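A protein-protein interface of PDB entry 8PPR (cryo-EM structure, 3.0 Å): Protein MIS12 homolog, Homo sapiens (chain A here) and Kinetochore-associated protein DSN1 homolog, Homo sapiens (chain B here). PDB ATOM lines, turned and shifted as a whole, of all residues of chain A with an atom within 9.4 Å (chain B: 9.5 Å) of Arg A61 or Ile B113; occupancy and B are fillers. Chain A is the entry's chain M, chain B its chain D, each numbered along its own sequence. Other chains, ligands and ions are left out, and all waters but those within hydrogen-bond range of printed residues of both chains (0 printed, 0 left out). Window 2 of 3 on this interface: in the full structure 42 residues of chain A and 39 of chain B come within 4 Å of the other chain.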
ATOM      1  N   MET A  36      19.325   7.234   9.987  1.00  0.00           N
ATOM      2  CA  MET A  36      18.073   6.486   9.993  1.00  0.00           C
ATOM      3  C   MET A  36      18.175   5.261  10.900  1.00  0.00           C
ATOM      4  O   MET A  36      17.210   4.912  11.588  1.00  0.00           O
ATOM      5  CB  MET A  36      17.684   6.121   8.558  1.00  0.00           C
ATOM      6  CG  MET A  36      16.351   5.394   8.397  1.00  0.00           C
ATOM      7  SD  MET A  36      16.406   3.621   8.689  1.00  0.00           S
ATOM      8  CE  MET A  36      17.274   3.113   7.213  1.00  0.00           C
ATOM      9  N   GLN A  37      19.347   4.620  10.946  1.00  0.00           N
ATOM     10  CA  GLN A  37      19.580   3.538  11.897  1.00  0.00           C
ATOM     11  C   GLN A  37      19.512   4.034  13.334  1.00  0.00           C
ATOM     12  O   GLN A  37      18.990   3.335  14.210  1.00  0.00           O
ATOM     13  CB  GLN A  37      20.938   2.889  11.628  1.00  0.00           C
ATOM     14  CG  GLN A  37      21.197   1.607  12.407  1.00  0.00           C
ATOM     15  CD  GLN A  37      20.497   0.405  11.814  1.00  0.00           C
ATOM     16  OE1 GLN A  37      21.075  -0.334  11.018  1.00  0.00           O
ATOM     17  NE2 GLN A  37      19.248   0.195  12.207  1.00  0.00           N
ATOM     18  N   ALA A  38      20.058   5.221  13.604  1.00  0.00           N
ATOM     19  CA  ALA A  38      19.985   5.770  14.954  1.00  0.00           C
ATOM     20  C   ALA A  38      18.541   6.033  15.357  1.00  0.00           C
ATOM     21  O   ALA A  38      18.138   5.747  16.491  1.00  0.00           O
ATOM     22  CB  ALA A  38      20.814   7.049  15.045  1.00  0.00           C
ATOM     23  N   GLU A  40      15.966   4.430  14.153  1.00  0.00           N
ATOM     24  CA  GLU A  40      15.373   3.110  14.354  1.00  0.00           C
ATOM     25  C   GLU A  40      15.723   2.551  15.728  1.00  0.00           C
ATOM     26  O   GLU A  40      14.866   1.986  16.416  1.00  0.00           O
ATOM     27  CB  GLU A  40      15.836   2.151  13.257  1.00  0.00           C
ATOM     28  CG  GLU A  40      15.489   0.695  13.534  1.00  0.00           C
ATOM     29  CD  GLU A  40      16.158  -0.267  12.573  1.00  0.00           C
ATOM     30  OE1 GLU A  40      16.481   0.144  11.439  1.00  0.00           O
ATOM     31  OE2 GLU A  40      16.359  -1.439  12.955  1.00  0.00           O
ATOM     32  N   GLN A  41      16.981   2.696  16.142  1.00  0.00           N
ATOM     33  CA  GLN A  41      17.380   2.229  17.465  1.00  0.00           C
ATOM     34  C   GLN A  41      16.629   2.983  18.554  1.00  0.00           C
ATOM     35  O   GLN A  41      16.206   2.391  19.553  1.00  0.00           O
ATOM     36  CB  GLN A  41      18.889   2.380  17.640  1.00  0.00           C
ATOM     37  CG  GLN A  41      19.708   1.415  16.797  1.00  0.00           C
ATOM     38  CD  GLN A  41      21.193   1.704  16.862  1.00  0.00           C
ATOM     39  OE1 GLN A  41      21.627   2.623  17.556  1.00  0.00           O
ATOM     40  NE2 GLN A  41      21.982   0.918  16.138  1.00  0.00           N
ATOM     41  N   ILE A  43      13.622   4.335  18.288  1.00  0.00           N
ATOM     42  CA  ILE A  43      12.217   3.937  18.315  1.00  0.00           C
ATOM     43  C   ILE A  43      12.062   2.541  18.913  1.00  0.00           C
ATOM     44  O   ILE A  43      11.109   2.278  19.659  1.00  0.00           O
ATOM     45  CB  ILE A  43      11.585   4.056  16.910  1.00  0.00           C
ATOM     46  CG1 ILE A  43      10.063   4.149  17.015  1.00  0.00           C
ATOM     47  CG2 ILE A  43      11.967   2.900  16.005  1.00  0.00           C
ATOM     48  CD1 ILE A  43       9.378   4.392  15.687  1.00  0.00           C
ATOM     49  N   LEU A  44      13.003   1.634  18.632  1.00  0.00           N
ATOM     50  CA  LEU A  44      12.944   0.313  19.257  1.00  0.00           C
ATOM     51  C   LEU A  44      13.195   0.384  20.760  1.00  0.00           C
ATOM     52  O   LEU A  44      12.557  -0.343  21.527  1.00  0.00           O
ATOM     53  CB  LEU A  44      13.918  -0.659  18.585  1.00  0.00           C
ATOM     54  CG  LEU A  44      13.483  -1.392  17.305  1.00  0.00           C
ATOM     55  CD1 LEU A  44      12.311  -2.310  17.624  1.00  0.00           C
ATOM     56  CD2 LEU A  44      13.115  -0.474  16.159  1.00  0.00           C
ATOM     57  N   LEU A  47      10.003   1.620  22.264  1.00  0.00           N
ATOM     58  CA  LEU A  47       9.032   0.530  22.309  1.00  0.00           C
ATOM     59  C   LEU A  47       9.361  -0.449  23.429  1.00  0.00           C
ATOM     60  O   LEU A  47       8.459  -0.977  24.090  1.00  0.00           O
ATOM     61  CB  LEU A  47       8.990  -0.186  20.960  1.00  0.00           C
ATOM     62  CG  LEU A  47       8.122   0.468  19.884  1.00  0.00           C
ATOM     63  CD1 LEU A  47       8.403  -0.142  18.518  1.00  0.00           C
ATOM     64  CD2 LEU A  47       6.652   0.336  20.245  1.00  0.00           C
ATOM     65  N   ASP A  48      10.650  -0.715  23.646  1.00  0.00           N
ATOM     66  CA  ASP A  48      11.056  -1.585  24.744  1.00  0.00           C
ATOM     67  C   ASP A  48      10.768  -0.948  26.097  1.00  0.00           C
ATOM     68  O   ASP A  48      10.527  -1.663  27.077  1.00  0.00           O
ATOM     69  CB  ASP A  48      12.542  -1.921  24.622  1.00  0.00           C
ATOM     70  CG  ASP A  48      12.839  -2.825  23.443  1.00  0.00           C
ATOM     71  OD1 ASP A  48      11.961  -3.633  23.076  1.00  0.00           O
ATOM     72  OD2 ASP A  48      13.950  -2.726  22.883  1.00  0.00           O
ATOM     73  N   ILE A  55       3.952  -3.378  18.878  1.00  0.00           N
ATOM     74  CA  ILE A  55       4.645  -3.071  17.630  1.00  0.00           C
ATOM     75  C   ILE A  55       5.856  -3.997  17.545  1.00  0.00           C
ATOM     76  O   ILE A  55       6.891  -3.745  18.163  1.00  0.00           O
ATOM     77  CB  ILE A  55       5.051  -1.598  17.547  1.00  0.00           C
ATOM     78  CG1 ILE A  55       3.867  -0.702  17.912  1.00  0.00           C
ATOM     79  CG2 ILE A  55       5.570  -1.265  16.155  1.00  0.00           C
ATOM     80  CD1 ILE A  55       2.656  -0.904  17.030  1.00  0.00           C
ATOM     81  N   SER A  56       5.725  -5.075  16.777  1.00  0.00           N
ATOM     82  CA  SER A  56       6.809  -6.032  16.646  1.00  0.00           C
ATOM     83  C   SER A  56       7.988  -5.408  15.902  1.00  0.00           C
ATOM     84  O   SER A  56       7.805  -4.516  15.069  1.00  0.00           O
ATOM     85  CB  SER A  56       6.334  -7.281  15.908  1.00  0.00           C
ATOM     86  OG  SER A  56       6.331  -7.073  14.507  1.00  0.00           O
ATOM     87  N   PRO A  57       9.212  -5.848  16.203  1.00  0.00           N
ATOM     88  CA  PRO A  57      10.372  -5.350  15.444  1.00  0.00           C
ATOM     89  C   PRO A  57      10.253  -5.586  13.950  1.00  0.00           C
ATOM     90  O   PRO A  57      10.775  -4.791  13.161  1.00  0.00           O
ATOM     91  CB  PRO A  57      11.555  -6.134  16.037  1.00  0.00           C
ATOM     92  CG  PRO A  57      11.028  -6.883  17.225  1.00  0.00           C
ATOM     93  CD  PRO A  57       9.600  -6.518  17.454  1.00  0.00           C
ATOM     94  N   VAL A  58       9.578  -6.663  13.539  1.00  0.00           N
ATOM     95  CA  VAL A  58       9.423  -6.952  12.115  1.00  0.00           C
ATOM     96  C   VAL A  58       8.618  -5.852  11.433  1.00  0.00           C
ATOM     97  O   VAL A  58       8.977  -5.377  10.349  1.00  0.00           O
ATOM     98  CB  VAL A  58       8.771  -8.332  11.921  1.00  0.00           C
ATOM     99  CG1 VAL A  58       8.582  -8.631  10.444  1.00  0.00           C
ATOM    100  CG2 VAL A  58       9.607  -9.411  12.594  1.00  0.00           C
ATOM    101  N   GLN A  59       7.517  -5.428  12.059  1.00  0.00           N
ATOM    102  CA  GLN A  59       6.662  -4.412  11.453  1.00  0.00           C
ATOM    103  C   GLN A  59       7.383  -3.075  11.331  1.00  0.00           C
ATOM    104  O   GLN A  59       7.340  -2.428  10.275  1.00  0.00           O
ATOM    105  CB  GLN A  59       5.383  -4.253  12.273  1.00  0.00           C
ATOM    106  CG  GLN A  59       4.439  -5.438  12.191  1.00  0.00           C
ATOM    107  CD  GLN A  59       3.358  -5.391  13.252  1.00  0.00           C
ATOM    108  OE1 GLN A  59       2.220  -5.793  13.014  1.00  0.00           O
ATOM    109  NE2 GLN A  59       3.710  -4.898  14.434  1.00  0.00           N
ATOM    110  N   ILE A  60       8.051  -2.642  12.403  1.00  0.00           N
ATOM    111  CA  ILE A  60       8.753  -1.365  12.360  1.00  0.00           C
ATOM    112  C   ILE A  60       9.924  -1.433  11.387  1.00  0.00           C
ATOM    113  O   ILE A  60      10.236  -0.450  10.711  1.00  0.00           O
ATOM    114  CB  ILE A  60       9.192  -0.935  13.774  1.00  0.00           C
ATOM    115  CG1 ILE A  60       9.738   0.495  13.752  1.00  0.00           C
ATOM    116  CG2 ILE A  60      10.219  -1.893  14.351  1.00  0.00           C
ATOM    117  CD1 ILE A  60       8.745   1.519  13.248  1.00  0.00           C
ATOM    118  N   ARG A  61      10.580  -2.593  11.286  1.00  0.00           N
ATOM    119  CA  ARG A  61      11.656  -2.731  10.310  1.00  0.00           C
ATOM    120  C   ARG A  61      11.127  -2.671   8.882  1.00  0.00           C
ATOM    121  O   ARG A  61      11.762  -2.072   8.010  1.00  0.00           O
ATOM    122  CB  ARG A  61      12.438  -4.022  10.545  1.00  0.00           C
ATOM    123  CG  ARG A  61      13.507  -4.271   9.489  1.00  0.00           C
ATOM    124  CD  ARG A  61      14.510  -3.126   9.412  1.00  0.00           C
ATOM    125  NE  ARG A  61      15.329  -3.000  10.611  1.00  0.00           N
ATOM    126  CZ  ARG A  61      16.483  -3.626  10.796  1.00  0.00           C
ATOM    127  NH1 ARG A  61      16.983  -4.439   9.879  1.00  0.00           N
ATOM    128  NH2 ARG A  61      17.155  -3.427  11.926  1.00  0.00           N
ATOM    129  N   LYS A  62       9.970  -3.283   8.620  1.00  0.00           N
ATOM    130  CA  LYS A  62       9.374  -3.175   7.290  1.00  0.00           C
ATOM    131  C   LYS A  62       9.014  -1.730   6.967  1.00  0.00           C
ATOM    132  O   LYS A  62       9.245  -1.254   5.847  1.00  0.00           O
ATOM    133  CB  LYS A  62       8.140  -4.071   7.188  1.00  0.00           C
ATOM    134  CG  LYS A  62       8.439  -5.560   7.252  1.00  0.00           C
ATOM    135  CD  LYS A  62       7.247  -6.381   6.785  1.00  0.00           C
ATOM    136  CE  LYS A  62       6.040  -6.169   7.686  1.00  0.00           C
ATOM    137  NZ  LYS A  62       6.240  -6.755   9.039  1.00  0.00           N
ATOM    138  N   CYS A  63       8.448  -1.015   7.943  1.00  0.00           N
ATOM    139  CA  CYS A  63       8.116   0.390   7.730  1.00  0.00           C
ATOM    140  C   CYS A  63       9.369   1.219   7.462  1.00  0.00           C
ATOM    141  O   CYS A  63       9.384   2.066   6.558  1.00  0.00           O
ATOM    142  CB  CYS A  63       7.357   0.933   8.939  1.00  0.00           C
ATOM    143  SG  CYS A  63       5.744   0.163   9.215  1.00  0.00           S
ATOM    144  N   THR A  64      10.433   0.981   8.233  1.00  0.00           N
ATOM    145  CA  THR A  64      11.679   1.709   8.021  1.00  0.00           C
ATOM    146  C   THR A  64      12.294   1.368   6.672  1.00  0.00           C
ATOM    147  O   THR A  64      12.886   2.233   6.026  1.00  0.00           O
ATOM    148  CB  THR A  64      12.671   1.421   9.147  1.00  0.00           C
ATOM    149  OG1 THR A  64      12.818   0.006   9.312  1.00  0.00           O
ATOM    150  CG2 THR A  64      12.196   2.040  10.454  1.00  0.00           C
ATOM    151  N   GLU A  65      12.179   0.112   6.235  1.00  0.00           N
ATOM    152  CA  GLU A  65      12.684  -0.265   4.918  1.00  0.00           C
ATOM    153  C   GLU A  65      11.920   0.446   3.808  1.00  0.00           C
ATOM    154  O   GLU A  65      12.522   0.921   2.838  1.00  0.00           O
ATOM    155  CB  GLU A  65      12.601  -1.780   4.738  1.00  0.00           C
ATOM    156  CG  GLU A  65      13.702  -2.556   5.437  1.00  0.00           C
ATOM    157  CD  GLU A  65      13.253  -3.941   5.858  1.00  0.00           C
ATOM    158  OE1 GLU A  65      12.042  -4.228   5.761  1.00  0.00           O
ATOM    159  OE2 GLU A  65      14.110  -4.742   6.288  1.00  0.00           O
ATOM    160  N   LYS A  66      10.593   0.529   3.934  1.00  0.00           N
ATOM    161  CA  LYS A  66       9.804   1.254   2.941  1.00  0.00           C
ATOM    162  C   LYS A  66      10.186   2.730   2.906  1.00  0.00           C
ATOM    163  O   LYS A  66      10.355   3.319   1.830  1.00  0.00           O
ATOM    164  CB  LYS A  66       8.313   1.101   3.248  1.00  0.00           C
ATOM    165  CG  LYS A  66       7.388   1.474   2.099  1.00  0.00           C
ATOM    166  CD  LYS A  66       7.627   0.605   0.872  1.00  0.00           C
ATOM    167  CE  LYS A  66       7.388  -0.867   1.177  1.00  0.00           C
ATOM    168  NZ  LYS A  66       7.937  -1.748   0.110  1.00  0.00           N
ATOM    169  N   PHE A  67      10.332   3.340   4.082  1.00  0.00           N
ATOM    170  CA  PHE A  67      10.646   4.763   4.162  1.00  0.00           C
ATOM    171  C   PHE A  67      12.071   5.021   3.671  1.00  0.00           C
ATOM    172  O   PHE A  67      12.349   6.039   3.020  1.00  0.00           O
ATOM    173  CB  PHE A  67      10.400   5.205   5.610  1.00  0.00           C
ATOM    174  CG  PHE A  67      10.612   6.661   5.882  1.00  0.00           C
ATOM    175  CD1 PHE A  67       9.675   7.594   5.470  1.00  0.00           C
ATOM    176  CD2 PHE A  67      11.665   7.090   6.669  1.00  0.00           C
ATOM    177  CE1 PHE A  67       9.834   8.936   5.752  1.00  0.00           C
ATOM    178  CE2 PHE A  67      11.828   8.433   6.964  1.00  0.00           C
ATOM    179  CZ  PHE A  67      10.915   9.358   6.500  1.00  0.00           C
ATOM    180  N   LEU A  68      12.973   4.067   3.923  1.00  0.00           N
ATOM    181  CA  LEU A  68      14.323   4.113   3.374  1.00  0.00           C
ATOM    182  C   LEU A  68      14.309   4.039   1.857  1.00  0.00           C
ATOM    183  O   LEU A  68      15.070   4.746   1.196  1.00  0.00           O
ATOM    184  CB  LEU A  68      15.157   2.964   3.944  1.00  0.00           C
ATOM    185  CG  LEU A  68      16.560   2.790   3.354  1.00  0.00           C
ATOM    186  CD1 LEU A  68      17.406   4.035   3.569  1.00  0.00           C
ATOM    187  CD2 LEU A  68      17.253   1.553   3.913  1.00  0.00           C
ATOM    188  N   CYS A  69      13.476   3.168   1.285  1.00  0.00           N
ATOM    189  CA  CYS A  69      13.376   3.094  -0.170  1.00  0.00           C
ATOM    190  C   CYS A  69      12.825   4.396  -0.741  1.00  0.00           C
ATOM    191  O   CYS A  69      13.249   4.847  -1.814  1.00  0.00           O
ATOM    192  CB  CYS A  69      12.504   1.908  -0.579  1.00  0.00           C
ATOM    193  SG  CYS A  69      12.371   1.655  -2.365  1.00  0.00           S
ATOM    194  N   SER B 109      23.312  -1.785   3.298  1.00  0.00           N
ATOM    195  CA  SER B 109      22.095  -2.416   3.787  1.00  0.00           C
ATOM    196  C   SER B 109      22.003  -2.247   5.297  1.00  0.00           C
ATOM    197  O   SER B 109      23.019  -2.143   5.989  1.00  0.00           O
ATOM    198  CB  SER B 109      22.045  -3.902   3.415  1.00  0.00           C
ATOM    199  OG  SER B 109      23.059  -4.633   4.081  1.00  0.00           O
ATOM    200  N   LEU B 110      20.770  -2.224   5.796  1.00  0.00           N
ATOM    201  CA  LEU B 110      20.536  -2.083   7.226  1.00  0.00           C
ATOM    202  C   LEU B 110      20.991  -3.322   7.983  1.00  0.00           C
ATOM    203  O   LEU B 110      20.842  -4.451   7.507  1.00  0.00           O
ATOM    204  CB  LEU B 110      19.055  -1.836   7.502  1.00  0.00           C
ATOM    205  CG  LEU B 110      18.546  -0.405   7.393  1.00  0.00           C
ATOM    206  CD1 LEU B 110      17.031  -0.395   7.481  1.00  0.00           C
ATOM    207  CD2 LEU B 110      19.161   0.419   8.505  1.00  0.00           C
ATOM    208  N   HIS B 111      21.548  -3.104   9.170  1.00  0.00           N
ATOM    209  CA  HIS B 111      21.872  -4.220  10.042  1.00  0.00           C
ATOM    210  C   HIS B 111      20.585  -4.815  10.609  1.00  0.00           C
ATOM    211  O   HIS B 111      19.729  -4.080  11.115  1.00  0.00           O
ATOM    212  CB  HIS B 111      22.793  -3.770  11.175  1.00  0.00           C
ATOM    213  CG  HIS B 111      24.224  -3.624  10.762  1.00  0.00           C
ATOM    214  ND1 HIS B 111      24.706  -4.124   9.571  1.00  0.00           N
ATOM    215  CD2 HIS B 111      25.278  -3.037  11.378  1.00  0.00           C
ATOM    216  CE1 HIS B 111      25.993  -3.848   9.469  1.00  0.00           C
ATOM    217  NE2 HIS B 111      26.366  -3.191  10.553  1.00  0.00           N
ATOM    218  N   PRO B 112      20.410  -6.130  10.528  1.00  0.00           N
ATOM    219  CA  PRO B 112      19.185  -6.746  11.046  1.00  0.00           C
ATOM    220  C   PRO B 112      19.151  -6.727  12.567  1.00  0.00           C
ATOM    221  O   PRO B 112      20.177  -6.637  13.243  1.00  0.00           O
ATOM    222  CB  PRO B 112      19.243  -8.183  10.509  1.00  0.00           C
ATOM    223  CG  PRO B 112      20.414  -8.224   9.555  1.00  0.00           C
ATOM    224  CD  PRO B 112      21.331  -7.122   9.955  1.00  0.00           C
ATOM    225  N   ILE B 113      17.929  -6.807  13.102  1.00  0.00           N
ATOM    226  CA  ILE B 113      17.756  -6.873  14.551  1.00  0.00           C
ATOM    227  C   ILE B 113      18.388  -8.144  15.098  1.00  0.00           C
ATOM    228  O   ILE B 113      19.057  -8.128  16.139  1.00  0.00           O
ATOM    229  CB  ILE B 113      16.262  -6.789  14.926  1.00  0.00           C
ATOM    230  CG1 ILE B 113      15.642  -5.471  14.456  1.00  0.00           C
ATOM    231  CG2 ILE B 113      16.078  -6.958  16.428  1.00  0.00           C
ATOM    232  CD1 ILE B 113      14.944  -5.570  13.115  1.00  0.00           C
ATOM    233  N   HIS B 114      18.187  -9.262  14.407  1.00  0.00           N
ATOM    234  CA  HIS B 114      18.685 -10.546  14.873  1.00  0.00           C
ATOM    235  C   HIS B 114      20.208 -10.587  14.836  1.00  0.00           C
ATOM    236  O   HIS B 114      20.853  -9.969  13.983  1.00  0.00           O
ATOM    237  CB  HIS B 114      18.113 -11.676  14.018  1.00  0.00           C
ATOM    238  CG  HIS B 114      16.618 -11.681  13.948  1.00  0.00           C
ATOM    239  ND1 HIS B 114      15.828 -11.031  14.873  1.00  0.00           N
ATOM    240  CD2 HIS B 114      15.768 -12.249  13.061  1.00  0.00           C
ATOM    241  CE1 HIS B 114      14.556 -11.203  14.560  1.00  0.00           C
ATOM    242  NE2 HIS B 114      14.492 -11.938  13.464  1.00  0.00           N
ATOM    243  N   GLN B 115      20.782 -11.327  15.780  1.00  0.00           N
ATOM    244  CA  GLN B 115      22.221 -11.500  15.886  1.00  0.00           C
ATOM    245  C   GLN B 115      22.574 -12.975  15.746  1.00  0.00           C
ATOM    246  O   GLN B 115      21.790 -13.857  16.111  1.00  0.00           O
ATOM    247  CB  GLN B 115      22.749 -10.953  17.221  1.00  0.00           C
ATOM    248  CG  GLN B 115      22.298 -11.737  18.445  1.00  0.00           C
ATOM    249  CD  GLN B 115      20.934 -11.303  18.950  1.00  0.00           C
ATOM    250  OE1 GLN B 115      20.181 -10.631  18.244  1.00  0.00           O
ATOM    251  NE2 GLN B 115      20.609 -11.687  20.179  1.00  0.00           N
ATOM    252  N   GLY B 116      23.760 -13.236  15.201  1.00  0.00           N
ATOM    253  CA  GLY B 116      24.213 -14.591  14.976  1.00  0.00           C
ATOM    254  C   GLY B 116      23.680 -15.248  13.722  1.00  0.00           C
ATOM    255  O   GLY B 116      24.007 -16.414  13.469  1.00  0.00           O
ATOM    256  N   ILE B 117      22.867 -14.543  12.932  1.00  0.00           N
ATOM    257  CA  ILE B 117      22.359 -15.113  11.689  1.00  0.00           C
ATOM    258  C   ILE B 117      23.493 -15.322  10.694  1.00  0.00           C
ATOM    259  O   ILE B 117      23.486 -16.285   9.918  1.00  0.00           O
ATOM    260  CB  ILE B 117      21.246 -14.221  11.110  1.00  0.00           C
ATOM    261  CG1 ILE B 117      21.705 -12.763  11.044  1.00  0.00           C
ATOM    262  CG2 ILE B 117      19.983 -14.342  11.944  1.00  0.00           C
ATOM    263  CD1 ILE B 117      20.732 -11.851  10.335  1.00  0.00           C
ATOM    264  N   PHE B 144      16.025 -21.295  13.458  1.00  0.00           N
ATOM    265  CA  PHE B 144      16.196 -19.997  14.102  1.00  0.00           C
ATOM    266  C   PHE B 144      14.875 -19.244  14.172  1.00  0.00           C
ATOM    267  O   PHE B 144      14.558 -18.625  15.193  1.00  0.00           O
ATOM    268  CB  PHE B 144      17.247 -19.177  13.355  1.00  0.00           C
ATOM    269  CG  PHE B 144      17.279 -17.733  13.754  1.00  0.00           C
ATOM    270  CD1 PHE B 144      17.715 -17.359  15.013  1.00  0.00           C
ATOM    271  CD2 PHE B 144      16.870 -16.748  12.872  1.00  0.00           C
ATOM    272  CE1 PHE B 144      17.746 -16.030  15.385  1.00  0.00           C
ATOM    273  CE2 PHE B 144      16.897 -15.419  13.238  1.00  0.00           C
ATOM    274  CZ  PHE B 144      17.335 -15.059  14.496  1.00  0.00           C
ATOM    275  N   LYS B 148      12.944 -18.257  17.554  1.00  0.00           N
ATOM    276  CA  LYS B 148      12.639 -16.851  17.787  1.00  0.00           C
ATOM    277  C   LYS B 148      11.154 -16.642  18.054  1.00  0.00           C
ATOM    278  O   LYS B 148      10.780 -15.822  18.900  1.00  0.00           O
ATOM    279  CB  LYS B 148      13.091 -16.012  16.591  1.00  0.00           C
ATOM    280  CG  LYS B 148      12.909 -14.515  16.777  1.00  0.00           C
ATOM    281  CD  LYS B 148      13.725 -14.004  17.953  1.00  0.00           C
ATOM    282  CE  LYS B 148      14.079 -12.536  17.782  1.00  0.00           C
ATOM    283  NZ  LYS B 148      12.923 -11.740  17.285  1.00  0.00           N
ATOM    284  N   PHE B 152       8.162 -15.386  21.714  1.00  0.00           N
ATOM    285  CA  PHE B 152       7.575 -14.094  21.370  1.00  0.00           C
ATOM    286  C   PHE B 152       6.101 -14.029  21.752  1.00  0.00           C
ATOM    287  O   PHE B 152       5.628 -12.998  22.246  1.00  0.00           O
ATOM    288  CB  PHE B 152       7.755 -13.820  19.877  1.00  0.00           C
ATOM    289  CG  PHE B 152       7.863 -12.361  19.538  1.00  0.00           C
ATOM    290  CD1 PHE B 152       6.729 -11.609  19.280  1.00  0.00           C
ATOM    291  CD2 PHE B 152       9.100 -11.739  19.480  1.00  0.00           C
ATOM    292  CE1 PHE B 152       6.825 -10.267  18.969  1.00  0.00           C
ATOM    293  CE2 PHE B 152       9.203 -10.397  19.168  1.00  0.00           C
ATOM    294  CZ  PHE B 152       8.063  -9.659  18.913  1.00  0.00           C
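The side-chain amide oxygen of Gln A37 sits at hydrogen-bond distance from the backbone NH of His B111.
The backbone carbonyl oxygen (O) of His B111 sits at hydrogen-bond distance from the guanidinium group (NH2) of Arg A61, at 2.8 Å.
The side-chain amide nitrogen (NE2) of Gln A37 lies within hydrogen-bond range of the side-chain carboxylate (OE1) of Glu A40, at 2.9 Å.
The side-chain amide oxygen (OE1) of Gln B115 lies close to the backbone carbonyl oxygen (O) of Ile B113 (3.5 Å).
OE2 of Glu A40 lies within salt-bridge range of NE of Arg A61 (3.0 Å).
OG1 of Thr A64 lies within hydrogen-bond range of O of Arg A61 (2.7 Å).
Among the printed residues, merely in contact across the chains: Gln A37 with Leu B110, Arg A61 with Ile B113, Arg A61 with Pro B112, Met A36 with Leu B110, Pro A57 with Phe B152 and Glu A40 with Leu B110.
Ala A38 touches none of the printed residues of chain B.
Of the printed residues of chain B, Glu A40 touches Leu B110 (3.98 Å).
Leu A44 touches none of the printed residues of chain B.
No residue of chain B comes within 4 Å of Ile A60.
Of chain B, only His B111 (2.8 Å), Pro B112 (3.4 Å) and Ile B113 (3.3 Å) come within 4 Å of Arg A61.
Of the printed residues of chain A, His B111 touches Gln A37 and Arg A61.
Pro B112 touches just one residue of chain A: Arg A61 (3.4 Å).
Of chain A, only Arg A61 comes within 4 Å of Ile B113.
Of the printed residues of chain A, Phe B152 touches Pro A57.
The nearest residue of chain B that does not touch Arg A61 is Leu B110 (4.1 Å).
The nearest residue of chain A that does not touch Ile B113 is Pro A57 (4.2 Å).
The nearest printed residue of chain B that does not touch Pro A57 is Ile B113 (4.2 Å).
Printed residues of chain B that touch a printed residue of chain A: Leu B110, His B111, Pro B112, Ile B113 and Phe B152.
Hydrophobic or aromatic side chains of chain B within 4 Å of the printed part of chain A: Leu B110, His B111, Ile B113 and Phe B152.
Among the printed residues, 8 pairs touch across the chains.
Among the printed residues, no Asp or Glu carboxylate lies within 4 Å of a Lys or Arg side-chain nitrogen of the other chain.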
